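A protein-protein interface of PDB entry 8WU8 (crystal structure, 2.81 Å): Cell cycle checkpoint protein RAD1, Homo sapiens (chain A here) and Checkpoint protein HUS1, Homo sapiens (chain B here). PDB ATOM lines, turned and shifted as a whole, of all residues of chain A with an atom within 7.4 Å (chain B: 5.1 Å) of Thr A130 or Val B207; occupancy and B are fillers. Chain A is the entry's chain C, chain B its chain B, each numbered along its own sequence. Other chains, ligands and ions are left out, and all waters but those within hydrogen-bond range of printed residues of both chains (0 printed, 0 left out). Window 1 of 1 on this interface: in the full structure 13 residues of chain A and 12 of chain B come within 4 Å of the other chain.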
ATOM      1  N   VAL A  88     -26.127  38.252  14.579  1.00  0.00           N
ATOM      2  CA  VAL A  88     -25.969  36.803  14.494  1.00  0.00           C
ATOM      3  C   VAL A  88     -27.320  36.100  14.570  1.00  0.00           C
ATOM      4  O   VAL A  88     -27.625  35.227  13.754  1.00  0.00           O
ATOM      5  CB  VAL A  88     -25.060  36.270  15.613  1.00  0.00           C
ATOM      6  CG1 VAL A  88     -25.058  34.745  15.619  1.00  0.00           C
ATOM      7  CG2 VAL A  88     -23.648  36.814  15.453  1.00  0.00           C
ATOM      8  N   ASP A  91     -28.988  36.225  11.449  1.00  0.00           N
ATOM      9  CA  ASP A  91     -28.355  35.372  10.449  1.00  0.00           C
ATOM     10  C   ASP A  91     -28.896  33.953  10.568  1.00  0.00           C
ATOM     11  O   ASP A  91     -29.252  33.323   9.574  1.00  0.00           O
ATOM     12  CB  ASP A  91     -26.834  35.371  10.605  1.00  0.00           C
ATOM     13  CG  ASP A  91     -26.192  36.642  10.092  1.00  0.00           C
ATOM     14  OD1 ASP A  91     -26.822  37.338   9.269  1.00  0.00           O
ATOM     15  OD2 ASP A  91     -25.052  36.941  10.510  1.00  0.00           O
ATOM     16  N   CYS A  92     -28.960  33.466  11.803  1.00  0.00           N
ATOM     17  CA  CYS A  92     -29.426  32.116  12.083  1.00  0.00           C
ATOM     18  C   CYS A  92     -30.892  31.924  11.699  1.00  0.00           C
ATOM     19  O   CYS A  92     -31.270  30.884  11.158  1.00  0.00           O
ATOM     20  CB  CYS A  92     -29.227  31.787  13.564  1.00  0.00           C
ATOM     21  SG  CYS A  92     -27.507  31.836  14.112  1.00  0.00           S
ATOM     22  N   ILE A  95     -31.228  31.487   7.934  1.00  0.00           N
ATOM     23  CA  ILE A  95     -30.200  30.597   7.401  1.00  0.00           C
ATOM     24  C   ILE A  95     -30.697  29.693   6.269  1.00  0.00           C
ATOM     25  O   ILE A  95     -29.893  29.135   5.526  1.00  0.00           O
ATOM     26  CB  ILE A  95     -29.602  29.718   8.522  1.00  0.00           C
ATOM     27  CG1 ILE A  95     -28.155  29.343   8.197  1.00  0.00           C
ATOM     28  CG2 ILE A  95     -30.459  28.485   8.759  1.00  0.00           C
ATOM     29  CD1 ILE A  95     -27.384  28.831   9.385  1.00  0.00           C
ATOM     30  N   PHE A  96     -32.013  29.546   6.136  1.00  0.00           N
ATOM     31  CA  PHE A  96     -32.579  28.797   5.015  1.00  0.00           C
ATOM     32  C   PHE A  96     -33.037  29.750   3.915  1.00  0.00           C
ATOM     33  O   PHE A  96     -33.727  29.348   2.976  1.00  0.00           O
ATOM     34  CB  PHE A  96     -33.748  27.919   5.472  1.00  0.00           C
ATOM     35  CG  PHE A  96     -33.326  26.652   6.168  1.00  0.00           C
ATOM     36  CD1 PHE A  96     -32.675  25.646   5.469  1.00  0.00           C
ATOM     37  CD2 PHE A  96     -33.595  26.458   7.516  1.00  0.00           C
ATOM     38  CE1 PHE A  96     -32.287  24.476   6.103  1.00  0.00           C
ATOM     39  CE2 PHE A  96     -33.212  25.290   8.156  1.00  0.00           C
ATOM     40  CZ  PHE A  96     -32.557  24.296   7.449  1.00  0.00           C
ATOM     41  N   ALA A 107     -39.913  26.329  10.276  1.00  0.00           N
ATOM     42  CA  ALA A 107     -40.322  26.376  11.679  1.00  0.00           C
ATOM     43  C   ALA A 107     -39.149  26.706  12.604  1.00  0.00           C
ATOM     44  O   ALA A 107     -37.993  26.453  12.268  1.00  0.00           O
ATOM     45  CB  ALA A 107     -40.958  25.059  12.086  1.00  0.00           C
ATOM     46  N   LEU A 108     -39.452  27.264  13.774  1.00  0.00           N
ATOM     47  CA  LEU A 108     -38.415  27.650  14.728  1.00  0.00           C
ATOM     48  C   LEU A 108     -38.709  27.189  16.154  1.00  0.00           C
ATOM     49  O   LEU A 108     -39.779  27.454  16.699  1.00  0.00           O
ATOM     50  CB  LEU A 108     -38.221  29.170  14.719  1.00  0.00           C
ATOM     51  CG  LEU A 108     -37.402  29.775  15.866  1.00  0.00           C
ATOM     52  CD1 LEU A 108     -35.936  29.364  15.792  1.00  0.00           C
ATOM     53  CD2 LEU A 108     -37.532  31.286  15.875  1.00  0.00           C
ATOM     54  N   ARG A 109     -37.744  26.495  16.748  1.00  0.00           N
ATOM     55  CA  ARG A 109     -37.777  26.183  18.173  1.00  0.00           C
ATOM     56  C   ARG A 109     -36.716  27.003  18.893  1.00  0.00           C
ATOM     57  O   ARG A 109     -35.524  26.873  18.606  1.00  0.00           O
ATOM     58  CB  ARG A 109     -37.558  24.687  18.411  1.00  0.00           C
ATOM     59  CG  ARG A 109     -38.828  23.849  18.339  1.00  0.00           C
ATOM     60  CD  ARG A 109     -39.594  23.880  19.654  1.00  0.00           C
ATOM     61  NE  ARG A 109     -38.816  23.288  20.737  1.00  0.00           N
ATOM     62  CZ  ARG A 109     -39.288  23.051  21.957  1.00  0.00           C
ATOM     63  NH1 ARG A 109     -40.545  23.354  22.258  1.00  0.00           N
ATOM     64  NH2 ARG A 109     -38.501  22.505  22.877  1.00  0.00           N
ATOM     65  N   LEU A 121     -31.285  27.977  19.116  1.00  0.00           N
ATOM     66  CA  LEU A 121     -32.251  28.060  18.030  1.00  0.00           C
ATOM     67  C   LEU A 121     -32.317  26.744  17.274  1.00  0.00           C
ATOM     68  O   LEU A 121     -31.294  26.101  17.044  1.00  0.00           O
ATOM     69  CB  LEU A 121     -31.889  29.186  17.067  1.00  0.00           C
ATOM     70  CG  LEU A 121     -31.822  30.594  17.648  1.00  0.00           C
ATOM     71  CD1 LEU A 121     -31.104  31.510  16.674  1.00  0.00           C
ATOM     72  CD2 LEU A 121     -33.221  31.113  17.951  1.00  0.00           C
ATOM     73  N   PHE A 122     -33.524  26.349  16.886  1.00  0.00           N
ATOM     74  CA  PHE A 122     -33.703  25.163  16.061  1.00  0.00           C
ATOM     75  C   PHE A 122     -34.646  25.463  14.904  1.00  0.00           C
ATOM     76  O   PHE A 122     -35.795  25.857  15.107  1.00  0.00           O
ATOM     77  CB  PHE A 122     -34.226  24.003  16.902  1.00  0.00           C
ATOM     78  CG  PHE A 122     -33.451  23.783  18.166  1.00  0.00           C
ATOM     79  CD1 PHE A 122     -32.221  23.149  18.137  1.00  0.00           C
ATOM     80  CD2 PHE A 122     -33.947  24.218  19.384  1.00  0.00           C
ATOM     81  CE1 PHE A 122     -31.502  22.953  19.299  1.00  0.00           C
ATOM     82  CE2 PHE A 122     -33.234  24.019  20.550  1.00  0.00           C
ATOM     83  CZ  PHE A 122     -32.012  23.383  20.507  1.00  0.00           C
ATOM     84  N   LEU A 123     -34.147  25.284  13.686  1.00  0.00           N
ATOM     85  CA  LEU A 123     -34.913  25.613  12.493  1.00  0.00           C
ATOM     86  C   LEU A 123     -35.002  24.417  11.558  1.00  0.00           C
ATOM     87  O   LEU A 123     -34.036  23.675  11.390  1.00  0.00           O
ATOM     88  CB  LEU A 123     -34.292  26.809  11.764  1.00  0.00           C
ATOM     89  CG  LEU A 123     -34.225  28.120  12.551  1.00  0.00           C
ATOM     90  CD1 LEU A 123     -32.886  28.265  13.263  1.00  0.00           C
ATOM     91  CD2 LEU A 123     -34.495  29.309  11.645  1.00  0.00           C
ATOM     92  N   GLU A 124     -36.169  24.230  10.954  1.00  0.00           N
ATOM     93  CA  GLU A 124     -36.382  23.111  10.048  1.00  0.00           C
ATOM     94  C   GLU A 124     -37.073  23.582   8.778  1.00  0.00           C
ATOM     95  O   GLU A 124     -37.930  24.461   8.818  1.00  0.00           O
ATOM     96  CB  GLU A 124     -37.200  22.012  10.738  1.00  0.00           C
ATOM     97  CG  GLU A 124     -37.523  20.804   9.867  1.00  0.00           C
ATOM     98  CD  GLU A 124     -38.803  20.982   9.068  1.00  0.00           C
ATOM     99  OE1 GLU A 124     -39.681  21.750   9.514  1.00  0.00           O
ATOM    100  OE2 GLU A 124     -38.925  20.362   7.990  1.00  0.00           O
ATOM    101  N   GLU A 125     -36.681  22.997   7.650  1.00  0.00           N
ATOM    102  CA  GLU A 125     -37.305  23.280   6.365  1.00  0.00           C
ATOM    103  C   GLU A 125     -37.171  22.083   5.433  1.00  0.00           C
ATOM    104  O   GLU A 125     -36.082  21.794   4.940  1.00  0.00           O
ATOM    105  CB  GLU A 125     -36.681  24.515   5.715  1.00  0.00           C
ATOM    106  CG  GLU A 125     -37.250  24.837   4.339  1.00  0.00           C
ATOM    107  CD  GLU A 125     -36.188  25.317   3.363  1.00  0.00           C
ATOM    108  OE1 GLU A 125     -36.074  26.545   3.157  1.00  0.00           O
ATOM    109  OE2 GLU A 125     -35.468  24.463   2.802  1.00  0.00           O
ATOM    110  N   GLY A 127     -37.333  18.982   6.156  1.00  0.00           N
ATOM    111  CA  GLY A 127     -36.562  17.924   6.779  1.00  0.00           C
ATOM    112  C   GLY A 127     -35.186  18.373   7.228  1.00  0.00           C
ATOM    113  O   GLY A 127     -34.652  17.860   8.212  1.00  0.00           O
ATOM    114  N   VAL A 128     -34.607  19.330   6.510  1.00  0.00           N
ATOM    115  CA  VAL A 128     -33.281  19.838   6.846  1.00  0.00           C
ATOM    116  C   VAL A 128     -33.321  20.624   8.152  1.00  0.00           C
ATOM    117  O   VAL A 128     -34.089  21.575   8.286  1.00  0.00           O
ATOM    118  CB  VAL A 128     -32.717  20.732   5.724  1.00  0.00           C
ATOM    119  CG1 VAL A 128     -31.279  21.113   6.029  1.00  0.00           C
ATOM    120  CG2 VAL A 128     -32.804  20.018   4.385  1.00  0.00           C
ATOM    121  N   VAL A 129     -32.494  20.225   9.113  1.00  0.00           N
ATOM    122  CA  VAL A 129     -32.510  20.835  10.442  1.00  0.00           C
ATOM    123  C   VAL A 129     -31.219  21.600  10.753  1.00  0.00           C
ATOM    124  O   VAL A 129     -30.118  21.076  10.582  1.00  0.00           O
ATOM    125  CB  VAL A 129     -32.735  19.770  11.538  1.00  0.00           C
ATOM    126  CG1 VAL A 129     -32.533  20.365  12.922  1.00  0.00           C
ATOM    127  CG2 VAL A 129     -34.124  19.161  11.412  1.00  0.00           C
ATOM    128  N   THR A 130     -31.369  22.841  11.212  1.00  0.00           N
ATOM    129  CA  THR A 130     -30.236  23.669  11.612  1.00  0.00           C
ATOM    130  C   THR A 130     -30.282  24.003  13.102  1.00  0.00           C
ATOM    131  O   THR A 130     -31.287  24.508  13.602  1.00  0.00           O
ATOM    132  CB  THR A 130     -30.185  24.980  10.808  1.00  0.00           C
ATOM    133  OG1 THR A 130     -29.887  24.688   9.437  1.00  0.00           O
ATOM    134  CG2 THR A 130     -29.117  25.909  11.365  1.00  0.00           C
ATOM    135  N   VAL A 131     -29.189  23.723  13.803  1.00  0.00           N
ATOM    136  CA  VAL A 131     -29.117  23.950  15.242  1.00  0.00           C
ATOM    137  C   VAL A 131     -28.119  25.060  15.566  1.00  0.00           C
ATOM    138  O   VAL A 131     -26.971  25.024  15.122  1.00  0.00           O
ATOM    139  CB  VAL A 131     -28.720  22.661  15.990  1.00  0.00           C
ATOM    140  CG1 VAL A 131     -28.534  22.931  17.472  1.00  0.00           C
ATOM    141  CG2 VAL A 131     -29.765  21.581  15.768  1.00  0.00           C
ATOM    142  N   CYS A 132     -28.561  26.043  16.344  1.00  0.00           N
ATOM    143  CA  CYS A 132     -27.729  27.200  16.660  1.00  0.00           C
ATOM    144  C   CYS A 132     -27.503  27.359  18.154  1.00  0.00           C
ATOM    145  O   CYS A 132     -28.434  27.255  18.948  1.00  0.00           O
ATOM    146  CB  CYS A 132     -28.363  28.476  16.104  1.00  0.00           C
ATOM    147  SG  CYS A 132     -28.751  28.404  14.347  1.00  0.00           S
ATOM    148  N   LYS A 133     -26.256  27.616  18.530  1.00  0.00           N
ATOM    149  CA  LYS A 133     -25.918  27.937  19.907  1.00  0.00           C
ATOM    150  C   LYS A 133     -25.348  29.345  19.960  1.00  0.00           C
ATOM    151  O   LYS A 133     -24.236  29.577  19.500  1.00  0.00           O
ATOM    152  CB  LYS A 133     -24.913  26.930  20.473  1.00  0.00           C
ATOM    153  CG  LYS A 133     -24.525  27.185  21.924  1.00  0.00           C
ATOM    154  CD  LYS A 133     -23.373  26.291  22.355  1.00  0.00           C
ATOM    155  CE  LYS A 133     -22.076  26.696  21.671  1.00  0.00           C
ATOM    156  NZ  LYS A 133     -21.636  28.059  22.083  1.00  0.00           N
ATOM    157  N   ILE A 134     -26.113  30.287  20.505  1.00  0.00           N
ATOM    158  CA  ILE A 134     -25.657  31.670  20.600  1.00  0.00           C
ATOM    159  C   ILE A 134     -25.422  32.081  22.048  1.00  0.00           C
ATOM    160  O   ILE A 134     -26.364  32.188  22.834  1.00  0.00           O
ATOM    161  CB  ILE A 134     -26.665  32.649  19.966  1.00  0.00           C
ATOM    162  CG1 ILE A 134     -27.024  32.211  18.546  1.00  0.00           C
ATOM    163  CG2 ILE A 134     -26.097  34.057  19.949  1.00  0.00           C
ATOM    164  CD1 ILE A 134     -27.940  33.176  17.825  1.00  0.00           C
ATOM    165  N   MET B 179     -23.716  31.335   6.772  1.00  0.00           N
ATOM    166  CA  MET B 179     -22.595  30.871   7.586  1.00  0.00           C
ATOM    167  C   MET B 179     -21.325  31.676   7.311  1.00  0.00           C
ATOM    168  O   MET B 179     -20.531  31.918   8.218  1.00  0.00           O
ATOM    169  CB  MET B 179     -22.331  29.382   7.343  1.00  0.00           C
ATOM    170  CG  MET B 179     -23.354  28.441   7.965  1.00  0.00           C
ATOM    171  SD  MET B 179     -22.845  26.712   7.867  1.00  0.00           S
ATOM    172  CE  MET B 179     -24.167  25.910   8.769  1.00  0.00           C
ATOM    173  N   ILE B 182     -20.383  34.642   9.355  1.00  0.00           N
ATOM    174  CA  ILE B 182     -19.962  34.359  10.722  1.00  0.00           C
ATOM    175  C   ILE B 182     -18.524  33.841  10.782  1.00  0.00           C
ATOM    176  O   ILE B 182     -17.708  34.355  11.547  1.00  0.00           O
ATOM    177  CB  ILE B 182     -20.906  33.342  11.389  1.00  0.00           C
ATOM    178  CG1 ILE B 182     -22.308  33.945  11.549  1.00  0.00           C
ATOM    179  CG2 ILE B 182     -20.356  32.906  12.738  1.00  0.00           C
ATOM    180  CD1 ILE B 182     -23.322  32.996  12.148  1.00  0.00           C
ATOM    181  N   LEU B 198     -23.194  20.394   7.678  1.00  0.00           N
ATOM    182  CA  LEU B 198     -22.413  21.618   7.547  1.00  0.00           C
ATOM    183  C   LEU B 198     -22.297  22.255   8.929  1.00  0.00           C
ATOM    184  O   LEU B 198     -23.292  22.378   9.646  1.00  0.00           O
ATOM    185  CB  LEU B 198     -23.053  22.576   6.541  1.00  0.00           C
ATOM    186  CG  LEU B 198     -23.231  22.033   5.119  1.00  0.00           C
ATOM    187  CD1 LEU B 198     -23.875  23.077   4.217  1.00  0.00           C
ATOM    188  CD2 LEU B 198     -21.904  21.567   4.537  1.00  0.00           C
ATOM    189  N   LYS B 199     -21.086  22.655   9.303  1.00  0.00           N
ATOM    190  CA  LYS B 199     -20.800  22.974  10.698  1.00  0.00           C
ATOM    191  C   LYS B 199     -19.756  24.077  10.876  1.00  0.00           C
ATOM    192  O   LYS B 199     -18.663  24.002  10.319  1.00  0.00           O
ATOM    193  CB  LYS B 199     -20.341  21.700  11.413  1.00  0.00           C
ATOM    194  CG  LYS B 199     -20.188  21.818  12.911  1.00  0.00           C
ATOM    195  CD  LYS B 199     -20.140  20.432  13.532  1.00  0.00           C
ATOM    196  CE  LYS B 199     -20.097  20.496  15.047  1.00  0.00           C
ATOM    197  NZ  LYS B 199     -20.310  19.153  15.660  1.00  0.00           N
ATOM    198  N   ILE B 200     -20.100  25.097  11.657  1.00  0.00           N
ATOM    199  CA  ILE B 200     -19.168  26.176  11.981  1.00  0.00           C
ATOM    200  C   ILE B 200     -19.119  26.406  13.484  1.00  0.00           C
ATOM    201  O   ILE B 200     -20.115  26.199  14.171  1.00  0.00           O
ATOM    202  CB  ILE B 200     -19.552  27.502  11.284  1.00  0.00           C
ATOM    203  CG1 ILE B 200     -20.969  27.921  11.667  1.00  0.00           C
ATOM    204  CG2 ILE B 200     -19.430  27.375   9.779  1.00  0.00           C
ATOM    205  CD1 ILE B 200     -21.400  29.233  11.047  1.00  0.00           C
ATOM    206  N   VAL B 205     -20.815  31.837  18.833  1.00  0.00           N
ATOM    207  CA  VAL B 205     -21.900  31.109  18.181  1.00  0.00           C
ATOM    208  C   VAL B 205     -21.455  29.814  17.493  1.00  0.00           C
ATOM    209  O   VAL B 205     -20.387  29.758  16.883  1.00  0.00           O
ATOM    210  CB  VAL B 205     -22.616  32.024  17.151  1.00  0.00           C
ATOM    211  CG1 VAL B 205     -21.617  32.579  16.153  1.00  0.00           C
ATOM    212  CG2 VAL B 205     -23.745  31.288  16.447  1.00  0.00           C
ATOM    213  N   CYS B 206     -22.279  28.775  17.623  1.00  0.00           N
ATOM    214  CA  CYS B 206     -22.094  27.527  16.893  1.00  0.00           C
ATOM    215  C   CYS B 206     -23.328  27.211  16.057  1.00  0.00           C
ATOM    216  O   CYS B 206     -24.457  27.386  16.511  1.00  0.00           O
ATOM    217  CB  CYS B 206     -21.794  26.378  17.855  1.00  0.00           C
ATOM    218  SG  CYS B 206     -20.167  26.480  18.610  1.00  0.00           S
ATOM    219  N   VAL B 207     -23.105  26.761  14.827  1.00  0.00           N
ATOM    220  CA  VAL B 207     -24.197  26.408  13.927  1.00  0.00           C
ATOM    221  C   VAL B 207     -23.892  25.088  13.233  1.00  0.00           C
ATOM    222  O   VAL B 207     -22.801  24.898  12.691  1.00  0.00           O
ATOM    223  CB  VAL B 207     -24.447  27.490  12.853  1.00  0.00           C
ATOM    224  CG1 VAL B 207     -25.599  27.082  11.946  1.00  0.00           C
ATOM    225  CG2 VAL B 207     -24.728  28.838  13.493  1.00  0.00           C
ATOM    226  N   THR B 208     -24.859  24.178  13.263  1.00  0.00           N
ATOM    227  CA  THR B 208     -24.754  22.908  12.559  1.00  0.00           C
ATOM    228  C   THR B 208     -26.026  22.658  11.756  1.00  0.00           C
ATOM    229  O   THR B 208     -27.126  22.645  12.309  1.00  0.00           O
ATOM    230  CB  THR B 208     -24.516  21.722  13.529  1.00  0.00           C
ATOM    231  OG1 THR B 208     -25.714  21.453  14.268  1.00  0.00           O
ATOM    232  CG2 THR B 208     -23.384  22.025  14.497  1.00  0.00           C
ATOM    233  N   THR B 209     -25.875  22.471  10.450  1.00  0.00           N
ATOM    234  CA  THR B 209     -27.006  22.147   9.593  1.00  0.00           C
ATOM    235  C   THR B 209     -26.995  20.658   9.269  1.00  0.00           C
ATOM    236  O   THR B 209     -25.955  20.113   8.905  1.00  0.00           O
ATOM    237  CB  THR B 209     -26.976  22.964   8.291  1.00  0.00           C
ATOM    238  OG1 THR B 209     -26.984  24.359   8.611  1.00  0.00           O
ATOM    239  CG2 THR B 209     -28.182  22.647   7.424  1.00  0.00           C
ATOM    240  N   HIS B 210     -28.146  20.002   9.408  1.00  0.00           N
ATOM    241  CA  HIS B 210     -28.237  18.560   9.178  1.00  0.00           C
ATOM    242  C   HIS B 210     -29.013  18.215   7.914  1.00  0.00           C
ATOM    243  O   HIS B 210     -30.203  18.514   7.803  1.00  0.00           O
ATOM    244  CB  HIS B 210     -28.895  17.860  10.370  1.00  0.00           C
ATOM    245  CG  HIS B 210     -28.092  17.919  11.633  1.00  0.00           C
ATOM    246  ND1 HIS B 210     -28.340  18.838  12.627  1.00  0.00           N
ATOM    247  CD2 HIS B 210     -27.054  17.163  12.064  1.00  0.00           C
ATOM    248  CE1 HIS B 210     -27.484  18.651  13.619  1.00  0.00           C
ATOM    249  NE2 HIS B 210     -26.697  17.642  13.303  1.00  0.00           N
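N of Lys A133 lies within hydrogen-bond range of O of Cys B206 (2.7 Å).
The side-chain hydroxyl of Thr A130 is in hydrogen-bond range of the side-chain hydroxyl of Thr B209, 3.0 Å away.
O of Thr B208 is in hydrogen-bond range of N of Val A131 (2.8 Å).
O of Val A129 is in hydrogen-bond range of N of His B210, at 2.5 Å.
The side-chain sulfur (SG) of Cys A92 lies within hydrogen-bond range of the backbone carbonyl oxygen (O) of Val A88, 3.4 Å away.
O of Leu A121 sits at hydrogen-bond distance from N of Cys A132.
The backbone carbonyl oxygen (O) of Leu B198 lies within hydrogen-bond range of the backbone NH (N) of Thr B209, at 2.7 Å.
The backbone NH (N) of Ile B200 is in hydrogen-bond range of the backbone carbonyl oxygen (O) of Val B207, at 2.9 Å.
The side-chain sulfur (SG) of Cys A132 lies close to the side-chain sulfur (SG) of Cys A92, at 3.7 Å.
The backbone carbonyl oxygen (O) of Leu A123 sits at hydrogen-bond distance from the backbone NH (N) of Thr A130 (2.8 Å).
CG1 of Val A88 touches CG2 of Val B205 (3.8 Å).
Thr B209 touches Val A128.
O of Val A129 touches O of Thr B208 (3.8 Å).
Thr B209 touches Val A129.
Val B207 touches Thr A130.
Thr A130 touches Thr B208 (CA to O, 3.3 Å).
Cys B206 touches Val A131 (O to O, 3.7 Å).
Val B207 touches Val A131.
Cys B206 touches Cys A132 (O to CA, 3.3 Å).
Val B205 touches Lys A133.
Of chain A, only Ile A95 (3.6 Å), Thr A130 (3.8 Å) and Val A131 (3.3 Å) come within 4 Å of Val B207.
Of the printed residues of chain B, Val A88 touches Val B205 (3.8 Å).
Printed residues of chain B within 4 Å of Val A129: Thr B208 (3.8 Å), Thr B209 (3.4 Å) and His B210 (2.5 Å).
Of the printed residues of chain B, Cys A132 touches Cys B206.
Of the printed residues of chain A, Cys B206 touches Val A131, Cys A132 and Lys A133.
Printed residues of chain B within 4 Å of Ile A95: Val B207.
Phe A122 touches none of the printed residues of chain B.
The nearest residue of chain B that does not touch Thr A130 is His B210 (4.7 Å).
The nearest printed residue of chain B that does not touch Lys A133 is Val B207 (4.9 Å).
Of the 11 printed residues of chain B, 6 touch a printed residue of chain A.
Hydrophobic or aromatic side chains of chain B within 4 Å of the printed part of chain A: Val B205, Val B207 and His B210.
Printed residues of chain A that touch a printed residue of chain B: Val A88, Ile A95, Val A128, Val A129, Thr A130, Val A131, Cys A132 and Lys A133.
Hydrophobic or aromatic side chains of chain A that line the printed part of chain B: Val A88, Ile A95, Val A128 and Val A131.
Among the printed residues, 16 pairs touch across the chains.
Among the printed residues, no Asp or Glu carboxylate lies within 4 Å of a Lys or Arg side-chain nitrogen of the other chain.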
